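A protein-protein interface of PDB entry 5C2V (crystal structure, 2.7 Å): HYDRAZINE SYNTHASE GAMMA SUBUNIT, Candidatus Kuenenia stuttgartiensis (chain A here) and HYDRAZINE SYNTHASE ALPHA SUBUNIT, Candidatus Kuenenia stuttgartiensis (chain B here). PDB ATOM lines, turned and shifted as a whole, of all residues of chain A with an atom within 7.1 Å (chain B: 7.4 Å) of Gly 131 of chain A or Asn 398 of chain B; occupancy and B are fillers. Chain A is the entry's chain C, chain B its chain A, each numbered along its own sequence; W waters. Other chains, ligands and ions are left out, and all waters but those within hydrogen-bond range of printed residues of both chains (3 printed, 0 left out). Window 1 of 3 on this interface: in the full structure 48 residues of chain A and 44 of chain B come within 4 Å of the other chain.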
ATOM      1  N   LEU A  24       9.353 -27.672   1.039  1.00  0.00           N
ATOM      2  CA  LEU A  24       8.862 -26.580   0.211  1.00  0.00           C
ATOM      3  C   LEU A  24       8.978 -25.240   0.925  1.00  0.00           C
ATOM      4  O   LEU A  24       8.884 -25.170   2.148  1.00  0.00           O
ATOM      5  CB  LEU A  24       7.402 -26.825  -0.179  1.00  0.00           C
ATOM      6  CG  LEU A  24       7.107 -27.942  -1.178  1.00  0.00           C
ATOM      7  CD1 LEU A  24       5.631 -28.305  -1.141  1.00  0.00           C
ATOM      8  CD2 LEU A  24       7.517 -27.507  -2.573  1.00  0.00           C
ATOM      9  N   THR A  25       9.199 -24.179   0.157  1.00  0.00           N
ATOM     10  CA  THR A  25       9.051 -22.829   0.683  1.00  0.00           C
ATOM     11  C   THR A  25       7.568 -22.473   0.682  1.00  0.00           C
ATOM     12  O   THR A  25       6.789 -23.061  -0.068  1.00  0.00           O
ATOM     13  CB  THR A  25       9.839 -21.794  -0.138  1.00  0.00           C
ATOM     14  OG1 THR A  25       9.183 -21.569  -1.391  1.00  0.00           O
ATOM     15  CG2 THR A  25      11.261 -22.275  -0.384  1.00  0.00           C
ATOM     16  N   VAL A  26       7.174 -21.532   1.533  1.00  0.00           N
ATOM     17  CA  VAL A  26       5.792 -21.058   1.556  1.00  0.00           C
ATOM     18  C   VAL A  26       5.336 -20.492   0.197  1.00  0.00           C
ATOM     19  O   VAL A  26       4.209 -20.762  -0.228  1.00  0.00           O
ATOM     20  CB  VAL A  26       5.578 -19.993   2.658  1.00  0.00           C
ATOM     21  CG1 VAL A  26       4.137 -19.504   2.661  1.00  0.00           C
ATOM     22  CG2 VAL A  26       5.947 -20.561   4.016  1.00  0.00           C
ATOM     23  N   PRO A  27       6.197 -19.711  -0.495  1.00  0.00           N
ATOM     24  CA  PRO A  27       5.784 -19.319  -1.848  1.00  0.00           C
ATOM     25  C   PRO A  27       5.571 -20.512  -2.779  1.00  0.00           C
ATOM     26  O   PRO A  27       4.692 -20.460  -3.638  1.00  0.00           O
ATOM     27  CB  PRO A  27       6.952 -18.458  -2.334  1.00  0.00           C
ATOM     28  CG  PRO A  27       7.533 -17.895  -1.097  1.00  0.00           C
ATOM     29  CD  PRO A  27       7.411 -18.985  -0.074  1.00  0.00           C
ATOM     30  N   TRP A  55       7.080 -35.616  12.919  1.00  0.00           N
ATOM     31  CA  TRP A  55       7.518 -34.601  11.970  1.00  0.00           C
ATOM     32  C   TRP A  55       7.404 -33.203  12.565  1.00  0.00           C
ATOM     33  O   TRP A  55       8.063 -32.268  12.108  1.00  0.00           O
ATOM     34  CB  TRP A  55       6.698 -34.681  10.682  1.00  0.00           C
ATOM     35  CG  TRP A  55       5.342 -34.068  10.823  1.00  0.00           C
ATOM     36  CD1 TRP A  55       4.209 -34.681  11.263  1.00  0.00           C
ATOM     37  CD2 TRP A  55       4.980 -32.714  10.532  1.00  0.00           C
ATOM     38  NE1 TRP A  55       3.158 -33.793  11.262  1.00  0.00           N
ATOM     39  CE2 TRP A  55       3.608 -32.577  10.817  1.00  0.00           C
ATOM     40  CE3 TRP A  55       5.684 -31.602  10.057  1.00  0.00           C
ATOM     41  CZ2 TRP A  55       2.924 -31.376  10.643  1.00  0.00           C
ATOM     42  CZ3 TRP A  55       5.006 -30.412   9.885  1.00  0.00           C
ATOM     43  CH2 TRP A  55       3.639 -30.307  10.176  1.00  0.00           C
ATOM     44  N   CYS A 126      -3.251 -27.838   3.871  1.00  0.00           N
ATOM     45  CA  CYS A 126      -2.302 -28.633   4.645  1.00  0.00           C
ATOM     46  C   CYS A 126      -0.867 -28.143   4.505  1.00  0.00           C
ATOM     47  O   CYS A 126      -0.121 -28.131   5.480  1.00  0.00           O
ATOM     48  CB  CYS A 126      -2.379 -30.100   4.231  1.00  0.00           C
ATOM     49  SG  CYS A 126      -3.944 -30.872   4.640  1.00  0.00           S
ATOM     50  N   GLY A 127      -0.483 -27.747   3.295  1.00  0.00           N
ATOM     51  CA  GLY A 127       0.867 -27.277   3.039  1.00  0.00           C
ATOM     52  C   GLY A 127       1.225 -26.045   3.848  1.00  0.00           C
ATOM     53  O   GLY A 127       2.399 -25.768   4.093  1.00  0.00           O
ATOM     54  N   ARG A 128       0.202 -25.304   4.261  1.00  0.00           N
ATOM     55  CA  ARG A 128       0.382 -24.115   5.085  1.00  0.00           C
ATOM     56  C   ARG A 128       0.590 -24.454   6.559  1.00  0.00           C
ATOM     57  O   ARG A 128       1.345 -23.780   7.258  1.00  0.00           O
ATOM     58  CB  ARG A 128      -0.822 -23.186   4.936  1.00  0.00           C
ATOM     59  CG  ARG A 128      -0.521 -21.894   4.204  1.00  0.00           C
ATOM     60  CD  ARG A 128      -1.668 -20.914   4.342  1.00  0.00           C
ATOM     61  NE  ARG A 128      -1.244 -19.548   4.060  1.00  0.00           N
ATOM     62  CZ  ARG A 128      -1.568 -18.498   4.809  1.00  0.00           C
ATOM     63  NH1 ARG A 128      -2.321 -18.660   5.888  1.00  0.00           N
ATOM     64  NH2 ARG A 128      -1.137 -17.290   4.481  1.00  0.00           N
ATOM     65  N   ASP A 129      -0.083 -25.505   7.017  1.00  0.00           N
ATOM     66  CA  ASP A 129      -0.109 -25.876   8.433  1.00  0.00           C
ATOM     67  C   ASP A 129       1.253 -26.032   9.132  1.00  0.00           C
ATOM     68  O   ASP A 129       1.362 -25.699  10.312  1.00  0.00           O
ATOM     69  CB  ASP A 129      -0.909 -27.170   8.607  1.00  0.00           C
ATOM     70  CG  ASP A 129      -2.399 -26.960   8.416  1.00  0.00           C
ATOM     71  OD1 ASP A 129      -2.850 -25.797   8.491  1.00  0.00           O
ATOM     72  OD2 ASP A 129      -3.119 -27.956   8.192  1.00  0.00           O
ATOM     73  N   PRO A 130       2.283 -26.559   8.436  1.00  0.00           N
ATOM     74  CA  PRO A 130       3.581 -26.601   9.120  1.00  0.00           C
ATOM     75  C   PRO A 130       4.084 -25.239   9.591  1.00  0.00           C
ATOM     76  O   PRO A 130       4.675 -25.168  10.664  1.00  0.00           O
ATOM     77  CB  PRO A 130       4.513 -27.175   8.053  1.00  0.00           C
ATOM     78  CG  PRO A 130       3.640 -28.055   7.255  1.00  0.00           C
ATOM     79  CD  PRO A 130       2.313 -27.348   7.190  1.00  0.00           C
ATOM     80  N   GLY A 131       3.881 -24.186   8.807  1.00  0.00           N
ATOM     81  CA  GLY A 131       4.320 -22.870   9.234  1.00  0.00           C
ATOM     82  C   GLY A 131       3.292 -22.022   9.962  1.00  0.00           C
ATOM     83  O   GLY A 131       3.657 -21.175  10.777  1.00  0.00           O
ATOM     84  N   PHE A 132       2.011 -22.233   9.674  1.00  0.00           N
ATOM     85  CA  PHE A 132       0.968 -21.417  10.293  1.00  0.00           C
ATOM     86  C   PHE A 132       0.240 -22.075  11.467  1.00  0.00           C
ATOM     87  O   PHE A 132      -0.553 -21.423  12.147  1.00  0.00           O
ATOM     88  CB  PHE A 132      -0.052 -21.001   9.229  1.00  0.00           C
ATOM     89  CG  PHE A 132       0.525 -20.128   8.149  1.00  0.00           C
ATOM     90  CD1 PHE A 132       1.240 -20.681   7.098  1.00  0.00           C
ATOM     91  CD2 PHE A 132       0.357 -18.753   8.187  1.00  0.00           C
ATOM     92  CE1 PHE A 132       1.774 -19.883   6.107  1.00  0.00           C
ATOM     93  CE2 PHE A 132       0.890 -17.949   7.196  1.00  0.00           C
ATOM     94  CZ  PHE A 132       1.599 -18.516   6.155  1.00  0.00           C
ATOM     95  N   VAL A 133       0.507 -23.354  11.716  1.00  0.00           N
ATOM     96  CA  VAL A 133      -0.147 -24.059  12.819  1.00  0.00           C
ATOM     97  C   VAL A 133       0.841 -24.864  13.660  1.00  0.00           C
ATOM     98  O   VAL A 133       1.065 -24.563  14.832  1.00  0.00           O
ATOM     99  CB  VAL A 133      -1.260 -25.002  12.314  1.00  0.00           C
ATOM    100  CG1 VAL A 133      -1.817 -25.833  13.464  1.00  0.00           C
ATOM    101  CG2 VAL A 133      -2.373 -24.204  11.649  1.00  0.00           C
ATOM    102  N   PHE A 134       1.418 -25.896  13.050  1.00  0.00           N
ATOM    103  CA  PHE A 134       2.347 -26.789  13.736  1.00  0.00           C
ATOM    104  C   PHE A 134       3.640 -26.082  14.133  1.00  0.00           C
ATOM    105  O   PHE A 134       4.299 -26.482  15.094  1.00  0.00           O
ATOM    106  CB  PHE A 134       2.675 -27.996  12.854  1.00  0.00           C
ATOM    107  CG  PHE A 134       1.558 -28.996  12.743  1.00  0.00           C
ATOM    108  CD1 PHE A 134       0.576 -28.859  11.774  1.00  0.00           C
ATOM    109  CD2 PHE A 134       1.499 -30.082  13.600  1.00  0.00           C
ATOM    110  CE1 PHE A 134      -0.448 -29.783  11.669  1.00  0.00           C
ATOM    111  CE2 PHE A 134       0.479 -31.010  13.499  1.00  0.00           C
ATOM    112  CZ  PHE A 134      -0.496 -30.860  12.533  1.00  0.00           C
ATOM    113  N   ARG A 135       3.988 -25.040  13.383  1.00  0.00           N
ATOM    114  CA  ARG A 135       5.236 -24.300  13.575  1.00  0.00           C
ATOM    115  C   ARG A 135       6.441 -25.231  13.473  1.00  0.00           C
ATOM    116  O   ARG A 135       7.363 -25.167  14.287  1.00  0.00           O
ATOM    117  CB  ARG A 135       5.237 -23.566  14.918  1.00  0.00           C
ATOM    118  CG  ARG A 135       3.952 -22.810  15.209  1.00  0.00           C
ATOM    119  CD  ARG A 135       3.638 -21.782  14.132  1.00  0.00           C
ATOM    120  NE  ARG A 135       2.444 -21.005  14.460  1.00  0.00           N
ATOM    121  CZ  ARG A 135       2.066 -19.903  13.819  1.00  0.00           C
ATOM    122  NH1 ARG A 135       2.790 -19.438  12.809  1.00  0.00           N
ATOM    123  NH2 ARG A 135       0.967 -19.262  14.193  1.00  0.00           N
ATOM    124  N   SER A 136       6.419 -26.099  12.466  1.00  0.00           N
ATOM    125  CA  SER A 136       7.505 -27.043  12.227  1.00  0.00           C
ATOM    126  C   SER A 136       7.992 -26.947  10.783  1.00  0.00           C
ATOM    127  O   SER A 136       7.572 -26.062  10.037  1.00  0.00           O
ATOM    128  CB  SER A 136       7.057 -28.472  12.544  1.00  0.00           C
ATOM    129  OG  SER A 136       8.139 -29.382  12.442  1.00  0.00           O
ATOM    130  N   GLU A 137       8.886 -27.852  10.398  1.00  0.00           N
ATOM    131  CA  GLU A 137       9.454 -27.854   9.053  1.00  0.00           C
ATOM    132  C   GLU A 137       8.394 -28.123   7.988  1.00  0.00           C
ATOM    133  O   GLU A 137       7.506 -28.956   8.177  1.00  0.00           O
ATOM    134  CB  GLU A 137      10.571 -28.894   8.950  1.00  0.00           C
ATOM    135  CG  GLU A 137      11.390 -28.802   7.674  1.00  0.00           C
ATOM    136  CD  GLU A 137      12.574 -29.748   7.674  1.00  0.00           C
ATOM    137  OE1 GLU A 137      12.369 -30.960   7.900  1.00  0.00           O
ATOM    138  OE2 GLU A 137      13.711 -29.279   7.456  1.00  0.00           O
ATOM    139  N   ASN A 138       8.496 -27.414   6.868  1.00  0.00           N
ATOM    140  CA  ASN A 138       7.552 -27.567   5.767  1.00  0.00           C
ATOM    141  C   ASN A 138       7.645 -28.936   5.101  1.00  0.00           C
ATOM    142  O   ASN A 138       8.675 -29.606   5.173  1.00  0.00           O
ATOM    143  CB  ASN A 138       7.775 -26.476   4.718  1.00  0.00           C
ATOM    144  CG  ASN A 138       7.346 -25.106   5.199  1.00  0.00           C
ATOM    145  OD1 ASN A 138       6.436 -24.979   6.017  1.00  0.00           O
ATOM    146  ND2 ASN A 138       7.998 -24.069   4.686  1.00  0.00           N
ATOM    147  N   TYR B 131      23.397 -22.709   9.670  1.00  0.00           N
ATOM    148  CA  TYR B 131      22.002 -23.080   9.852  1.00  0.00           C
ATOM    149  C   TYR B 131      21.390 -23.275   8.485  1.00  0.00           C
ATOM    150  O   TYR B 131      21.285 -22.326   7.719  1.00  0.00           O
ATOM    151  CB  TYR B 131      21.242 -22.009  10.633  1.00  0.00           C
ATOM    152  CG  TYR B 131      19.812 -22.380  10.957  1.00  0.00           C
ATOM    153  CD1 TYR B 131      19.519 -23.218  12.024  1.00  0.00           C
ATOM    154  CD2 TYR B 131      18.755 -21.886  10.202  1.00  0.00           C
ATOM    155  CE1 TYR B 131      18.215 -23.559  12.328  1.00  0.00           C
ATOM    156  CE2 TYR B 131      17.445 -22.221  10.499  1.00  0.00           C
ATOM    157  CZ  TYR B 131      17.183 -23.058  11.564  1.00  0.00           C
ATOM    158  OH  TYR B 131      15.885 -23.397  11.869  1.00  0.00           O
ATOM    159  N   ILE B 201      13.254 -18.105   0.503  1.00  0.00           N
ATOM    160  CA  ILE B 201      12.355 -18.482   1.592  1.00  0.00           C
ATOM    161  C   ILE B 201      11.136 -17.561   1.704  1.00  0.00           C
ATOM    162  O   ILE B 201      10.005 -18.015   1.885  1.00  0.00           O
ATOM    163  CB  ILE B 201      13.108 -18.480   2.940  1.00  0.00           C
ATOM    164  CG1 ILE B 201      14.301 -19.435   2.883  1.00  0.00           C
ATOM    165  CG2 ILE B 201      12.177 -18.856   4.076  1.00  0.00           C
ATOM    166  CD1 ILE B 201      15.164 -19.408   4.124  1.00  0.00           C
ATOM    167  N   ASN B 263      14.698 -18.613  18.065  1.00  0.00           N
ATOM    168  CA  ASN B 263      14.604 -18.918  16.642  1.00  0.00           C
ATOM    169  C   ASN B 263      15.744 -18.249  15.885  1.00  0.00           C
ATOM    170  O   ASN B 263      16.356 -17.305  16.386  1.00  0.00           O
ATOM    171  CB  ASN B 263      13.254 -18.479  16.075  1.00  0.00           C
ATOM    172  CG  ASN B 263      12.101 -19.307  16.605  1.00  0.00           C
ATOM    173  OD1 ASN B 263      12.173 -19.867  17.698  1.00  0.00           O
ATOM    174  ND2 ASN B 263      11.026 -19.389  15.827  1.00  0.00           N
ATOM    175  N   TRP B 264      16.040 -18.738  14.685  1.00  0.00           N
ATOM    176  CA  TRP B 264      17.167 -18.209  13.923  1.00  0.00           C
ATOM    177  C   TRP B 264      16.904 -16.781  13.445  1.00  0.00           C
ATOM    178  O   TRP B 264      17.832 -16.079  13.044  1.00  0.00           O
ATOM    179  CB  TRP B 264      17.500 -19.126  12.740  1.00  0.00           C
ATOM    180  CG  TRP B 264      16.432 -19.233  11.692  1.00  0.00           C
ATOM    181  CD1 TRP B 264      15.250 -19.909  11.792  1.00  0.00           C
ATOM    182  CD2 TRP B 264      16.464 -18.674  10.373  1.00  0.00           C
ATOM    183  NE1 TRP B 264      14.538 -19.792  10.622  1.00  0.00           N
ATOM    184  CE2 TRP B 264      15.261 -19.039   9.735  1.00  0.00           C
ATOM    185  CE3 TRP B 264      17.389 -17.893   9.672  1.00  0.00           C
ATOM    186  CZ2 TRP B 264      14.961 -18.651   8.431  1.00  0.00           C
ATOM    187  CZ3 TRP B 264      17.088 -17.509   8.377  1.00  0.00           C
ATOM    188  CH2 TRP B 264      15.884 -17.888   7.770  1.00  0.00           C
ATOM    189  N   ASP B 265      15.643 -16.358  13.479  1.00  0.00           N
ATOM    190  CA  ASP B 265      15.306 -14.958  13.231  1.00  0.00           C
ATOM    191  C   ASP B 265      15.115 -14.177  14.534  1.00  0.00           C
ATOM    192  O   ASP B 265      14.893 -12.966  14.513  1.00  0.00           O
ATOM    193  CB  ASP B 265      14.050 -14.848  12.360  1.00  0.00           C
ATOM    194  CG  ASP B 265      12.890 -15.670  12.891  1.00  0.00           C
ATOM    195  OD1 ASP B 265      12.939 -16.094  14.064  1.00  0.00           O
ATOM    196  OD2 ASP B 265      11.922 -15.887  12.133  1.00  0.00           O
ATOM    197  N   ALA B 267      12.678 -14.713  16.834  1.00  0.00           N
ATOM    198  CA  ALA B 267      11.261 -14.448  17.055  1.00  0.00           C
ATOM    199  C   ALA B 267      10.742 -14.945  18.405  1.00  0.00           C
ATOM    200  O   ALA B 267       9.732 -14.445  18.901  1.00  0.00           O
ATOM    201  CB  ALA B 267      10.442 -15.068  15.930  1.00  0.00           C
ATOM    202  N   ARG B 395      15.897 -29.331  11.341  1.00  0.00           N
ATOM    203  CA  ARG B 395      14.810 -28.729  10.578  1.00  0.00           C
ATOM    204  C   ARG B 395      14.856 -27.205  10.645  1.00  0.00           C
ATOM    205  O   ARG B 395      15.150 -26.632  11.693  1.00  0.00           O
ATOM    206  CB  ARG B 395      13.460 -29.243  11.083  1.00  0.00           C
ATOM    207  CG  ARG B 395      13.187 -28.953  12.548  1.00  0.00           C
ATOM    208  CD  ARG B 395      12.075 -29.838  13.085  1.00  0.00           C
ATOM    209  NE  ARG B 395      12.465 -31.246  13.092  1.00  0.00           N
ATOM    210  CZ  ARG B 395      11.697 -32.233  13.539  1.00  0.00           C
ATOM    211  NH1 ARG B 395      10.489 -31.970  14.017  1.00  0.00           N
ATOM    212  NH2 ARG B 395      12.135 -33.483  13.507  1.00  0.00           N
ATOM    213  N   TRP B 396      14.576 -26.550   9.523  1.00  0.00           N
ATOM    214  CA  TRP B 396      14.566 -25.093   9.498  1.00  0.00           C
ATOM    215  C   TRP B 396      13.145 -24.563   9.657  1.00  0.00           C
ATOM    216  O   TRP B 396      12.210 -25.047   9.020  1.00  0.00           O
ATOM    217  CB  TRP B 396      15.204 -24.561   8.211  1.00  0.00           C
ATOM    218  CG  TRP B 396      14.457 -24.871   6.951  1.00  0.00           C
ATOM    219  CD1 TRP B 396      14.532 -26.017   6.212  1.00  0.00           C
ATOM    220  CD2 TRP B 396      13.541 -24.011   6.264  1.00  0.00           C
ATOM    221  NE1 TRP B 396      13.710 -25.928   5.116  1.00  0.00           N
ATOM    222  CE2 TRP B 396      13.090 -24.704   5.123  1.00  0.00           C
ATOM    223  CE3 TRP B 396      13.053 -22.723   6.505  1.00  0.00           C
ATOM    224  CZ2 TRP B 396      12.175 -24.156   4.228  1.00  0.00           C
ATOM    225  CZ3 TRP B 396      12.145 -22.179   5.615  1.00  0.00           C
ATOM    226  CH2 TRP B 396      11.715 -22.895   4.490  1.00  0.00           C
ATOM    227  N   ILE B 397      12.998 -23.564  10.521  1.00  0.00           N
ATOM    228  CA  ILE B 397      11.689 -23.036  10.883  1.00  0.00           C
ATOM    229  C   ILE B 397      11.309 -21.846  10.007  1.00  0.00           C
ATOM    230  O   ILE B 397      12.161 -21.033   9.648  1.00  0.00           O
ATOM    231  CB  ILE B 397      11.656 -22.613  12.368  1.00  0.00           C
ATOM    232  CG1 ILE B 397      12.296 -23.692  13.243  1.00  0.00           C
ATOM    233  CG2 ILE B 397      10.232 -22.327  12.823  1.00  0.00           C
ATOM    234  CD1 ILE B 397      11.569 -25.020  13.206  1.00  0.00           C
ATOM    235  N   ASN B 398      10.029 -21.759   9.658  1.00  0.00           N
ATOM    236  CA  ASN B 398       9.523 -20.656   8.848  1.00  0.00           C
ATOM    237  C   ASN B 398       9.741 -19.297   9.505  1.00  0.00           C
ATOM    238  O   ASN B 398       9.495 -19.129  10.699  1.00  0.00           O
ATOM    239  CB  ASN B 398       8.035 -20.853   8.554  1.00  0.00           C
ATOM    240  CG  ASN B 398       7.782 -21.946   7.537  1.00  0.00           C
ATOM    241  OD1 ASN B 398       7.916 -21.730   6.331  1.00  0.00           O
ATOM    242  ND2 ASN B 398       7.413 -23.128   8.015  1.00  0.00           N
ATOM    243  N   THR B 399      10.203 -18.332   8.716  1.00  0.00           N
ATOM    244  CA  THR B 399      10.455 -16.987   9.218  1.00  0.00           C
ATOM    245  C   THR B 399       9.457 -15.978   8.658  1.00  0.00           C
ATOM    246  O   THR B 399       9.220 -15.915   7.450  1.00  0.00           O
ATOM    247  CB  THR B 399      11.887 -16.521   8.890  1.00  0.00           C
ATOM    248  OG1 THR B 399      12.016 -15.127   9.196  1.00  0.00           O
ATOM    249  CG2 THR B 399      12.205 -16.745   7.418  1.00  0.00           C
ATOM    250  N   PHE B 400       8.854 -15.203   9.550  1.00  0.00           N
ATOM    251  CA  PHE B 400       7.879 -14.197   9.154  1.00  0.00           C
ATOM    252  C   PHE B 400       8.474 -12.792   9.044  1.00  0.00           C
ATOM    253  O   PHE B 400       7.747 -11.820   8.841  1.00  0.00           O
ATOM    254  CB  PHE B 400       6.693 -14.221  10.117  1.00  0.00           C
ATOM    255  CG  PHE B 400       5.800 -15.413   9.922  1.00  0.00           C
ATOM    256  CD1 PHE B 400       6.051 -16.603  10.585  1.00  0.00           C
ATOM    257  CD2 PHE B 400       4.730 -15.351   9.046  1.00  0.00           C
ATOM    258  CE1 PHE B 400       5.235 -17.704  10.391  1.00  0.00           C
ATOM    259  CE2 PHE B 400       3.912 -16.448   8.849  1.00  0.00           C
ATOM    260  CZ  PHE B 400       4.165 -17.625   9.522  1.00  0.00           C
ATOM    261  N   THR B 401       9.791 -12.682   9.199  1.00  0.00           N
ATOM    262  CA  THR B 401      10.470 -11.411   8.960  1.00  0.00           C
ATOM    263  C   THR B 401      11.588 -11.535   7.924  1.00  0.00           C
ATOM    264  O   THR B 401      12.324 -12.523   7.891  1.00  0.00           O
ATOM    265  CB  THR B 401      11.062 -10.821  10.257  1.00  0.00           C
ATOM    266  OG1 THR B 401      11.862  -9.675   9.939  1.00  0.00           O
ATOM    267  CG2 THR B 401      11.924 -11.848  10.976  1.00  0.00           C
ATOM    268  N   TYR B 413       1.369 -14.080   2.739  1.00  0.00           N
ATOM    269  CA  TYR B 413       2.809 -14.262   2.922  1.00  0.00           C
ATOM    270  C   TYR B 413       3.580 -13.400   1.923  1.00  0.00           C
ATOM    271  O   TYR B 413       4.327 -13.907   1.085  1.00  0.00           O
ATOM    272  CB  TYR B 413       3.199 -15.738   2.779  1.00  0.00           C
ATOM    273  CG  TYR B 413       4.547 -16.084   3.379  1.00  0.00           C
ATOM    274  CD1 TYR B 413       4.684 -16.307   4.743  1.00  0.00           C
ATOM    275  CD2 TYR B 413       5.679 -16.195   2.581  1.00  0.00           C
ATOM    276  CE1 TYR B 413       5.912 -16.625   5.296  1.00  0.00           C
ATOM    277  CE2 TYR B 413       6.911 -16.511   3.124  1.00  0.00           C
ATOM    278  CZ  TYR B 413       7.021 -16.726   4.483  1.00  0.00           C
ATOM    279  OH  TYR B 413       8.244 -17.043   5.027  1.00  0.00           O
ATOM    280  N   HIS B 552       5.920  -8.948  14.426  1.00  0.00           N
ATOM    281  CA  HIS B 552       5.797 -10.117  15.295  1.00  0.00           C
ATOM    282  C   HIS B 552       5.025  -9.850  16.584  1.00  0.00           C
ATOM    283  O   HIS B 552       5.280  -8.868  17.282  1.00  0.00           O
ATOM    284  CB  HIS B 552       7.179 -10.658  15.656  1.00  0.00           C
ATOM    285  CG  HIS B 552       7.852 -11.396  14.541  1.00  0.00           C
ATOM    286  ND1 HIS B 552       8.031 -10.849  13.288  1.00  0.00           N
ATOM    287  CD2 HIS B 552       8.388 -12.635  14.494  1.00  0.00           C
ATOM    288  CE1 HIS B 552       8.651 -11.724  12.518  1.00  0.00           C
ATOM    289  NE2 HIS B 552       8.880 -12.816  13.221  1.00  0.00           N
HETATM  290  O   HOH W   1      10.292 -25.122   6.911  1.00  0.00           O
HETATM  291  O   HOH W   2       9.409 -20.395   3.105  1.00  0.00           O
HETATM  292  O   HOH W   3       7.719 -23.567  11.020  1.00  0.00           O
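O of Trp 55 of chain A is in hydrogen-bond range of NH1 of Arg 395 of chain B (3.1 Å). The side-chain amide oxygen of Asn 398 of chain B sits at hydrogen-bond distance from the side-chain amide nitrogen of Asn 138 of chain A, 2.9 Å away.
The side-chain hydroxyl (OH) of Tyr 413 of chain B sits at hydrogen-bond distance from the backbone carbonyl oxygen (O) of Thr 399 of chain B (2.8 Å). The guanidinium group (NH1) of Arg 135 of chain A is in hydrogen-bond range of the backbone carbonyl oxygen (O) of Gly 131 of chain A (2.8 Å). The guanidinium group (NH2) of Arg 135 of chain A lies within hydrogen-bond range of the backbone carbonyl oxygen (O) of Phe 132 of chain A, at 3.3 Å. The side-chain hydroxyl (OH) of Tyr 131 of chain B is in hydrogen-bond range of the backbone carbonyl oxygen (O) of Arg 395 of chain B, at 3.3 Å. O of Pro 130 of chain A is in hydrogen-bond range of N of Ser 136 of chain A. O of Leu 24 of chain A is in hydrogen-bond range of ND2 of Asn 138 of chain A.
Among the printed residues, merely in contact across the chains: Val 26 of chain A with Asn 398 of chain B (3.3 Å), Val 26 of chain A with Tyr 413 of chain B (3.5 Å), Pro 27 of chain A with Ile 201 of chain B (3.4 Å), Gly 131 of chain A with Asn 398 of chain B (3.3 Å), Gly 131 of chain A with Phe 400 of chain B (3.8 Å), Phe 132 of chain A with Phe 400 of chain B (3.8 Å), Arg 135 of chain A with Phe 400 of chain B (3.9 Å), Ser 136 of chain A with Arg 395 of chain B (3.8 Å), Ser 136 of chain A with Asn 398 of chain B (3.6 Å), Glu 137 of chain A with Arg 395 of chain B (3.4 Å), Glu 137 of chain A with Trp 396 of chain B (3.5 Å) and Asn 138 of chain A with Trp 396 of chain B (3.9 Å).
Gly 131 of chain A touches two residues of chain B. Of the printed residues of chain A, Arg 395 of chain B touches Trp 55 (3.1 Å), Ser 136 (3.8 Å) and Glu 137 (3.4 Å). Printed residues of chain B within 4 Å of Ser 136 of chain A: Arg 395 (3.8 Å) and Asn 398 (3.6 Å). Of the printed residues of chain B, Asn 138 of chain A touches Trp 396 and Asn 398. Cys 126 of chain A touches none of the printed residues of chain B. Asp 265 of chain B touches none of the printed residues of chain A. The nearest residue of chain B that does not touch Gly 131 of chain A is Ile 397 of chain B (6.9 Å). The nearest printed residue of chain B that does not touch Arg 135 of chain A is Ile 397 of chain B (4.3 Å).
Hydrophobic or aromatic side chains of chain A that line the printed part of chain B: Val 26, Pro 27 and Phe 132. Among the printed residues, 14 pairs touch across the chains. Among the printed residues, no Asp or Glu carboxylate lies within 4 Å of a Lys or Arg side-chain nitrogen of the other chain.
Water W3 lies within hydrogen-bond range of the backbone carbonyl oxygen (O) of Ser 136 of chain A (2.7 Å), the side-chain amide nitrogen (ND2) of Asn 398 of chain B (3.1 Å) and the backbone carbonyl oxygen (O) of Pro 130 of chain A (3.5 Å). Water W2 bridges O of Ile 201 of chain B and N of Val 26 of chain A. Water W1 bridges the backbone carbonyl oxygen of Trp 396 of chain B (2.9 Å) and the backbone NH of Asn 138 of chain A (2.9 Å).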
